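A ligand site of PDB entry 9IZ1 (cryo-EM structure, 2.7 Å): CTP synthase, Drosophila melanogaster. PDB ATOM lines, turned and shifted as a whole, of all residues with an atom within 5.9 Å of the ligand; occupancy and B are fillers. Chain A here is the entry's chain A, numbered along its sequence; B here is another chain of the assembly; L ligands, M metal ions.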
ATOM      1  N   GLY A  48      -5.420  36.576  25.631  1.00  0.00           N
ATOM      2  CA  GLY A  48      -5.656  35.164  25.832  1.00  0.00           C
ATOM      3  C   GLY A  48      -7.086  34.722  25.574  1.00  0.00           C
ATOM      4  O   GLY A  48      -7.338  33.519  25.477  1.00  0.00           O
ATOM      5  N   THR A  49      -8.010  35.661  25.450  1.00  0.00           N
ATOM      6  CA  THR A  49      -9.422  35.350  25.237  1.00  0.00           C
ATOM      7  C   THR A  49      -9.941  35.877  23.903  1.00  0.00           C
ATOM      8  O   THR A  49     -11.110  36.286  23.819  1.00  0.00           O
ATOM      9  CB  THR A  49     -10.260  35.919  26.390  1.00  0.00           C
ATOM     10  OG1 THR A  49      -9.944  37.304  26.581  1.00  0.00           O
ATOM     11  CG2 THR A  49      -9.968  35.155  27.668  1.00  0.00           C
ATOM     12  N   PHE A  50      -9.111  35.883  22.869  1.00  0.00           N
ATOM     13  CA  PHE A  50      -9.510  36.383  21.555  1.00  0.00           C
ATOM     14  C   PHE A  50      -9.777  35.237  20.591  1.00  0.00           C
ATOM     15  O   PHE A  50      -9.123  34.189  20.661  1.00  0.00           O
ATOM     16  CB  PHE A  50      -8.438  37.284  20.955  1.00  0.00           C
ATOM     17  CG  PHE A  50      -8.411  38.671  21.533  1.00  0.00           C
ATOM     18  CD1 PHE A  50      -9.174  39.000  22.634  1.00  0.00           C
ATOM     19  CD2 PHE A  50      -7.642  39.662  20.941  1.00  0.00           C
ATOM     20  CE1 PHE A  50      -9.147  40.275  23.153  1.00  0.00           C
ATOM     21  CE2 PHE A  50      -7.624  40.934  21.445  1.00  0.00           C
ATOM     22  CZ  PHE A  50      -8.371  41.238  22.562  1.00  0.00           C
ATOM     23  N   SER A  51     -10.740  35.442  19.701  1.00  0.00           N
ATOM     24  CA  SER A  51     -10.884  34.554  18.562  1.00  0.00           C
ATOM     25  C   SER A  51      -9.779  34.852  17.540  1.00  0.00           C
ATOM     26  O   SER A  51      -9.393  36.004  17.361  1.00  0.00           O
ATOM     27  CB  SER A  51     -12.258  34.730  17.906  1.00  0.00           C
ATOM     28  OG  SER A  51     -12.403  33.886  16.780  1.00  0.00           O
ATOM     29  N   PRO A  52      -9.268  33.826  16.860  1.00  0.00           N
ATOM     30  CA  PRO A  52      -8.252  34.070  15.824  1.00  0.00           C
ATOM     31  C   PRO A  52      -8.755  34.917  14.677  1.00  0.00           C
ATOM     32  O   PRO A  52      -7.932  35.476  13.933  1.00  0.00           O
ATOM     33  CB  PRO A  52      -7.864  32.665  15.374  1.00  0.00           C
ATOM     34  CG  PRO A  52      -8.230  31.783  16.521  1.00  0.00           C
ATOM     35  CD  PRO A  52      -9.458  32.392  17.114  1.00  0.00           C
ATOM     36  N   TYR A  53     -10.068  35.013  14.480  1.00  0.00           N
ATOM     37  CA  TYR A  53     -10.617  35.829  13.410  1.00  0.00           C
ATOM     38  C   TYR A  53     -10.568  37.318  13.709  1.00  0.00           C
ATOM     39  O   TYR A  53     -10.540  38.130  12.773  1.00  0.00           O
ATOM     40  CB  TYR A  53     -12.064  35.418  13.129  1.00  0.00           C
ATOM     41  CG  TYR A  53     -12.204  34.030  12.547  1.00  0.00           C
ATOM     42  CD1 TYR A  53     -11.703  33.729  11.294  1.00  0.00           C
ATOM     43  CD2 TYR A  53     -12.837  33.022  13.258  1.00  0.00           C
ATOM     44  CE1 TYR A  53     -11.833  32.456  10.758  1.00  0.00           C
ATOM     45  CE2 TYR A  53     -12.968  31.749  12.736  1.00  0.00           C
ATOM     46  CZ  TYR A  53     -12.464  31.478  11.482  1.00  0.00           C
ATOM     47  OH  TYR A  53     -12.597  30.212  10.952  1.00  0.00           O
ATOM     48  N   LYS A 306      -9.166  24.817  11.495  1.00  0.00           N
ATOM     49  CA  LYS A 306     -10.541  25.283  11.572  1.00  0.00           C
ATOM     50  C   LYS A 306     -10.683  26.796  11.417  1.00  0.00           C
ATOM     51  O   LYS A 306     -11.805  27.294  11.402  1.00  0.00           O
ATOM     52  CB  LYS A 306     -11.174  24.852  12.905  1.00  0.00           C
ATOM     53  CG  LYS A 306     -10.308  25.148  14.112  1.00  0.00           C
ATOM     54  CD  LYS A 306     -10.992  24.717  15.401  1.00  0.00           C
ATOM     55  CE  LYS A 306     -12.215  25.575  15.674  1.00  0.00           C
ATOM     56  NZ  LYS A 306     -12.927  25.141  16.912  1.00  0.00           N
ATOM     57  N   TYR A 307      -9.577  27.517  11.314  1.00  0.00           N
ATOM     58  CA  TYR A 307      -9.580  28.972  11.159  1.00  0.00           C
ATOM     59  C   TYR A 307      -9.065  29.384   9.780  1.00  0.00           C
ATOM     60  O   TYR A 307      -8.383  30.388   9.623  1.00  0.00           O
ATOM     61  CB  TYR A 307      -8.767  29.637  12.258  1.00  0.00           C
ATOM     62  CG  TYR A 307      -9.054  29.101  13.643  1.00  0.00           C
ATOM     63  CD1 TYR A 307     -10.202  29.478  14.326  1.00  0.00           C
ATOM     64  CD2 TYR A 307      -8.182  28.238  14.265  1.00  0.00           C
ATOM     65  CE1 TYR A 307     -10.468  28.993  15.588  1.00  0.00           C
ATOM     66  CE2 TYR A 307      -8.434  27.742  15.528  1.00  0.00           C
ATOM     67  CZ  TYR A 307      -9.574  28.128  16.190  1.00  0.00           C
ATOM     68  OH  TYR A 307      -9.838  27.636  17.446  1.00  0.00           O
ATOM     69  N   GLY A 372      -5.977  24.703  18.518  1.00  0.00           N
ATOM     70  CA  GLY A 372      -7.248  25.384  18.399  1.00  0.00           C
ATOM     71  C   GLY A 372      -8.083  25.145  19.633  1.00  0.00           C
ATOM     72  O   GLY A 372      -7.712  24.391  20.538  1.00  0.00           O
ATOM     73  N   PHE A 373      -9.238  25.804  19.661  1.00  0.00           N
ATOM     74  CA  PHE A 373     -10.167  25.696  20.773  1.00  0.00           C
ATOM     75  C   PHE A 373     -11.555  25.361  20.236  1.00  0.00           C
ATOM     76  O   PHE A 373     -11.891  25.644  19.081  1.00  0.00           O
ATOM     77  CB  PHE A 373     -10.214  26.987  21.593  1.00  0.00           C
ATOM     78  CG  PHE A 373      -8.908  27.308  22.284  1.00  0.00           C
ATOM     79  CD1 PHE A 373      -8.629  26.796  23.545  1.00  0.00           C
ATOM     80  CD2 PHE A 373      -7.963  28.102  21.669  1.00  0.00           C
ATOM     81  CE1 PHE A 373      -7.435  27.077  24.169  1.00  0.00           C
ATOM     82  CE2 PHE A 373      -6.760  28.385  22.294  1.00  0.00           C
ATOM     83  CZ  PHE A 373      -6.502  27.875  23.547  1.00  0.00           C
ATOM     84  N   GLY A 374     -12.367  24.745  21.103  1.00  0.00           N
ATOM     85  CA  GLY A 374     -13.697  24.331  20.726  1.00  0.00           C
ATOM     86  C   GLY A 374     -13.737  22.907  20.213  1.00  0.00           C
ATOM     87  O   GLY A 374     -12.739  22.177  20.169  1.00  0.00           O
ATOM     88  N   SER A 375     -14.944  22.501  19.805  1.00  0.00           N
ATOM     89  CA  SER A 375     -15.181  21.157  19.282  1.00  0.00           C
ATOM     90  C   SER A 375     -15.408  21.137  17.781  1.00  0.00           C
ATOM     91  O   SER A 375     -15.369  20.051  17.186  1.00  0.00           O
ATOM     92  CB  SER A 375     -16.384  20.512  19.988  1.00  0.00           C
ATOM     93  OG  SER A 375     -17.542  21.317  19.861  1.00  0.00           O
ATOM     94  N   ARG A 376     -15.640  22.283  17.156  1.00  0.00           N
ATOM     95  CA  ARG A 376     -15.884  22.321  15.723  1.00  0.00           C
ATOM     96  C   ARG A 376     -14.600  22.025  14.949  1.00  0.00           C
ATOM     97  O   ARG A 376     -13.545  22.591  15.247  1.00  0.00           O
ATOM     98  CB  ARG A 376     -16.447  23.684  15.319  1.00  0.00           C
ATOM     99  CG  ARG A 376     -15.991  24.199  13.962  1.00  0.00           C
ATOM    100  CD  ARG A 376     -16.516  25.601  13.707  1.00  0.00           C
ATOM    101  NE  ARG A 376     -15.645  26.348  12.808  1.00  0.00           N
ATOM    102  CZ  ARG A 376     -14.792  27.283  13.191  1.00  0.00           C
ATOM    103  NH1 ARG A 376     -14.648  27.607  14.465  1.00  0.00           N
ATOM    104  NH2 ARG A 376     -14.042  27.902  12.273  1.00  0.00           N
ATOM    105  N   GLU A 423     -12.824  18.132  27.153  1.00  0.00           N
ATOM    106  CA  GLU A 423     -13.178  19.424  26.574  1.00  0.00           C
ATOM    107  C   GLU A 423     -14.425  19.330  25.707  1.00  0.00           C
ATOM    108  O   GLU A 423     -15.237  20.266  25.679  1.00  0.00           O
ATOM    109  CB  GLU A 423     -12.008  19.967  25.744  1.00  0.00           C
ATOM    110  CG  GLU A 423     -12.252  21.321  25.103  1.00  0.00           C
ATOM    111  CD  GLU A 423     -11.142  21.710  24.135  1.00  0.00           C
ATOM    112  OE1 GLU A 423     -10.310  20.850  23.807  1.00  0.00           O
ATOM    113  OE2 GLU A 423     -11.116  22.882  23.709  1.00  0.00           O
ATOM    114  N   LEU A 444     -11.496  32.515  32.992  1.00  0.00           N
ATOM    115  CA  LEU A 444     -10.855  32.438  31.693  1.00  0.00           C
ATOM    116  C   LEU A 444     -10.004  33.678  31.441  1.00  0.00           C
ATOM    117  O   LEU A 444     -10.437  34.799  31.702  1.00  0.00           O
ATOM    118  CB  LEU A 444     -11.902  32.275  30.587  1.00  0.00           C
ATOM    119  CG  LEU A 444     -12.777  31.021  30.683  1.00  0.00           C
ATOM    120  CD1 LEU A 444     -13.852  31.042  29.612  1.00  0.00           C
ATOM    121  CD2 LEU A 444     -11.932  29.773  30.576  1.00  0.00           C
ATOM    122  N   GLY A 445      -8.791  33.472  30.938  1.00  0.00           N
ATOM    123  CA  GLY A 445      -7.870  34.563  30.701  1.00  0.00           C
ATOM    124  C   GLY A 445      -6.670  34.515  31.614  1.00  0.00           C
ATOM    125  O   GLY A 445      -6.756  34.892  32.794  1.00  0.00           O
ATOM    126  N   MET A 448      -4.100  29.172  32.111  1.00  0.00           N
ATOM    127  CA  MET A 448      -3.638  27.881  31.638  1.00  0.00           C
ATOM    128  C   MET A 448      -2.186  27.663  32.050  1.00  0.00           C
ATOM    129  O   MET A 448      -1.632  28.394  32.884  1.00  0.00           O
ATOM    130  CB  MET A 448      -3.776  27.795  30.115  1.00  0.00           C
ATOM    131  CG  MET A 448      -4.814  28.703  29.500  1.00  0.00           C
ATOM    132  SD  MET A 448      -5.380  28.043  27.920  1.00  0.00           S
ATOM    133  CE  MET A 448      -6.435  29.366  27.352  1.00  0.00           C
ATOM    134  N   ARG A 479       0.466  26.727  25.670  1.00  0.00           N
ATOM    135  CA  ARG A 479      -0.849  27.371  25.636  1.00  0.00           C
ATOM    136  C   ARG A 479      -1.945  26.299  25.668  1.00  0.00           C
ATOM    137  O   ARG A 479      -2.876  26.297  24.857  1.00  0.00           O
ATOM    138  CB  ARG A 479      -0.969  28.299  24.414  1.00  0.00           C
ATOM    139  CG  ARG A 479      -2.335  28.959  24.200  1.00  0.00           C
ATOM    140  CD  ARG A 479      -2.732  29.860  25.356  1.00  0.00           C
ATOM    141  NE  ARG A 479      -4.045  30.476  25.160  1.00  0.00           N
ATOM    142  CZ  ARG A 479      -4.391  31.259  24.141  1.00  0.00           C
ATOM    143  NH1 ARG A 479      -3.517  31.603  23.209  1.00  0.00           N
ATOM    144  NH2 ARG A 479      -5.627  31.725  24.081  1.00  0.00           N
ATOM    145  N   ARG A 481      -4.706  23.779  28.077  1.00  0.00           N
ATOM    146  CA  ARG A 481      -5.484  23.679  29.301  1.00  0.00           C
ATOM    147  C   ARG A 481      -5.895  22.250  29.646  1.00  0.00           C
ATOM    148  O   ARG A 481      -6.327  22.016  30.787  1.00  0.00           O
ATOM    149  CB  ARG A 481      -6.744  24.554  29.217  1.00  0.00           C
ATOM    150  CG  ARG A 481      -7.306  24.998  30.555  1.00  0.00           C
ATOM    151  CD  ARG A 481      -8.642  25.697  30.412  1.00  0.00           C
ATOM    152  NE  ARG A 481      -8.534  27.037  29.847  1.00  0.00           N
ATOM    153  CZ  ARG A 481      -8.417  28.147  30.566  1.00  0.00           C
ATOM    154  NH1 ARG A 481      -8.375  28.103  31.886  1.00  0.00           N
ATOM    155  NH2 ARG A 481      -8.356  29.318  29.943  1.00  0.00           N
ATOM    156  N   TYR A 482      -5.780  21.300  28.723  1.00  0.00           N
ATOM    157  CA  TYR A 482      -6.139  19.917  28.962  1.00  0.00           C
ATOM    158  C   TYR A 482      -4.917  19.023  28.712  1.00  0.00           C
ATOM    159  O   TYR A 482      -4.026  19.364  27.936  1.00  0.00           O
ATOM    160  CB  TYR A 482      -7.293  19.472  28.062  1.00  0.00           C
ATOM    161  CG  TYR A 482      -8.576  20.252  28.250  1.00  0.00           C
ATOM    162  CD1 TYR A 482      -8.758  21.484  27.623  1.00  0.00           C
ATOM    163  CD2 TYR A 482      -9.598  19.776  29.055  1.00  0.00           C
ATOM    164  CE1 TYR A 482      -9.922  22.206  27.790  1.00  0.00           C
ATOM    165  CE2 TYR A 482     -10.763  20.499  29.235  1.00  0.00           C
ATOM    166  CZ  TYR A 482     -10.918  21.708  28.596  1.00  0.00           C
ATOM    167  OH  TYR A 482     -12.082  22.431  28.777  1.00  0.00           O
ATOM    168  N   LEU B 107     -16.126  36.333  26.380  1.00  0.00           N
ATOM    169  CA  LEU B 107     -15.172  35.432  25.746  1.00  0.00           C
ATOM    170  C   LEU B 107     -15.327  35.452  24.224  1.00  0.00           C
ATOM    171  O   LEU B 107     -16.441  35.371  23.694  1.00  0.00           O
ATOM    172  CB  LEU B 107     -15.373  34.014  26.260  1.00  0.00           C
ATOM    173  CG  LEU B 107     -14.369  32.985  25.732  1.00  0.00           C
ATOM    174  CD1 LEU B 107     -12.964  33.343  26.205  1.00  0.00           C
ATOM    175  CD2 LEU B 107     -14.745  31.576  26.141  1.00  0.00           C
ATOM    176  N   GLY B 108     -14.201  35.558  23.530  1.00  0.00           N
ATOM    177  CA  GLY B 108     -14.195  35.469  22.082  1.00  0.00           C
ATOM    178  C   GLY B 108     -13.983  36.785  21.366  1.00  0.00           C
ATOM    179  O   GLY B 108     -13.261  36.845  20.362  1.00  0.00           O
ATOM    180  N   LYS B 109     -14.593  37.850  21.871  1.00  0.00           N
ATOM    181  CA  LYS B 109     -14.537  39.158  21.235  1.00  0.00           C
ATOM    182  C   LYS B 109     -13.721  40.112  22.090  1.00  0.00           C
ATOM    183  O   LYS B 109     -13.629  39.967  23.310  1.00  0.00           O
ATOM    184  CB  LYS B 109     -15.933  39.736  21.010  1.00  0.00           C
ATOM    185  CG  LYS B 109     -17.020  38.691  20.821  1.00  0.00           C
ATOM    186  CD  LYS B 109     -17.065  38.202  19.380  1.00  0.00           C
ATOM    187  CE  LYS B 109     -17.188  39.360  18.404  1.00  0.00           C
ATOM    188  NZ  LYS B 109     -17.984  38.994  17.201  1.00  0.00           N
HETATM  189  P1  LIG L   1     -15.810  28.370  17.526  1.00  0.00           P
HETATM  190  O1  LIG L   1     -16.723  28.879  18.601  1.00  0.00           O
HETATM  191  O2  LIG L   1     -16.408  28.685  16.170  1.00  0.00           O
HETATM  192  O3  LIG L   1     -15.649  26.868  17.660  1.00  0.00           O
HETATM  193  O4  LIG L   1     -14.336  29.088  17.655  1.00  0.00           O
HETATM  194  P2  LIG L   1     -13.295  28.788  18.891  1.00  0.00           P
HETATM  195  O5  LIG L   1     -13.788  27.593  19.678  1.00  0.00           O
HETATM  196  O6  LIG L   1     -11.928  28.510  18.347  1.00  0.00           O
HETATM  197  O7  LIG L   1     -13.223  30.083  19.906  1.00  0.00           O
HETATM  198  P3  LIG L   1     -14.089  31.474  19.739  1.00  0.00           P
HETATM  199  O8  LIG L   1     -13.973  31.994  18.335  1.00  0.00           O
HETATM  200  O9  LIG L   1     -15.538  31.215  20.067  1.00  0.00           O
HETATM  201  O10 LIG L   1     -13.476  32.554  20.816  1.00  0.00           O
HETATM  202  C1  LIG L   1     -12.899  32.019  21.967  1.00  0.00           C
HETATM  203  C2  LIG L   1     -11.581  32.420  22.131  1.00  0.00           C
HETATM  204  O11 LIG L   1     -11.248  32.389  23.659  1.00  0.00           O
HETATM  205  C3  LIG L   1     -10.617  31.398  21.495  1.00  0.00           C
HETATM  206  O12 LIG L   1     -10.029  31.953  20.255  1.00  0.00           O
HETATM  207  C4  LIG L   1      -9.649  31.171  22.380  1.00  0.00           C
HETATM  208  C5  LIG L   1     -10.030  31.949  23.760  1.00  0.00           C
HETATM  209  N1  LIG L   1      -9.880  31.107  24.930  1.00  0.00           N
HETATM  210  C6  LIG L   1      -9.164  31.032  26.069  1.00  0.00           C
HETATM  211  N2  LIG L   1      -9.568  29.943  26.755  1.00  0.00           N
HETATM  212  C7  LIG L   1     -10.523  29.348  26.059  1.00  0.00           C
HETATM  213  C8  LIG L   1     -11.339  28.089  26.355  1.00  0.00           C
HETATM  214  O13 LIG L   1     -11.140  27.471  27.349  1.00  0.00           O
HETATM  215  N3  LIG L   1     -12.337  27.641  25.432  1.00  0.00           N
HETATM  216  C9  LIG L   1     -12.567  28.395  24.227  1.00  0.00           C
HETATM  217  N4  LIG L   1     -13.579  27.963  23.282  1.00  0.00           N
HETATM  218  N5  LIG L   1     -11.780  29.603  23.960  1.00  0.00           N
HETATM  219  C10 LIG L   1     -10.736  30.073  24.919  1.00  0.00           C
HETATM  220 MG    MG M   1     -16.381  28.757  21.577  1.00  0.00          MG
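Gly 48 touches the ligand (O to C6, 3.1 Å).
C of Thr 49 touches O11 of the ligand, at 3.7 Å.
Pro 52 touches the ligand (CD to O12, 3.2 Å).
CE of Met 448 touches N2 of the ligand, at 3.2 Å.
Leu 107 of chain B touches the ligand.
Gly 108 of chain B touches the ligand.
Hydrophobic or aromatic side chains that line the ligand: Pro 52, Tyr 307, Phe 373, Met 448 and Leu 107 of chain B.
Within 4 Å of the ligand: Gly 48, Thr 49, Phe 50, Ser 51, Pro 52, Lys 306, Tyr 307, Phe 373, Gly 374, Arg 376, Met 448, Arg 481, Leu 107 of chain B and Gly 108 of chain B.
Along chain A the residues within 4 Å of the ligand span positions 48 to 481.
The nearest printed residue that does not touch the ligand is Leu 444 (4.04 Å).
The side-chain amino group (NZ) of Lys 306 lies within hydrogen-bond range of the backbone carbonyl oxygen (O) of Phe 373 (2.5 Å).
The side-chain hydroxyl (OH) of Tyr 53 sits at hydrogen-bond distance from the guanidinium group (NH2) of Arg 376.
The backbone carbonyl oxygen (O) of Gly 48 is in hydrogen-bond range of the guanidinium group (NH2) of Arg 479, at 2.8 Å.
The side-chain hydroxyl of Ser 51 sits close to the backbone NH of Tyr 53 (3.5 Å).
OH of Tyr 307 sits at hydrogen-bond distance from N of Phe 373, 2.9 Å away.
O of Lys 306 lies within hydrogen-bond range of OH of Tyr 53, at 3.1 Å.
N of Gly 108 of chain B is in hydrogen-bond range of O of Thr 49 (3.2 Å).
The side-chain carboxylate (OE2) of Glu 423 sits at hydrogen-bond distance from the backbone NH (N) of Gly 374.
A nitrogen (N2) of the ligand lies within hydrogen-bond range of the guanidinium group (NH2) of Arg 481.
The side-chain amino group (NZ) of Lys 306 is in salt-bridge range of an oxygen (O3) of the ligand, at 3.3 Å.
The backbone carbonyl oxygen (O) of Phe 373 sits close to an oxygen (O5) of the ligand (2.8 Å).
The backbone carbonyl oxygen (O) of Phe 50 is in hydrogen-bond range of an oxygen (O12) of the ligand, 2.4 Å away.
OH of Tyr 307 sits at hydrogen-bond distance from O6 of the ligand.
The guanidinium group of Arg 376 is in salt-bridge range of an oxygen (O2) of the ligand, at 2.7 Å.
N of Gly 374 sits close to O5 of the ligand (3.5 Å).
The side-chain hydroxyl of Ser 51 lies within hydrogen-bond range of an oxygen (O8) of the ligand, 2.9 Å away.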
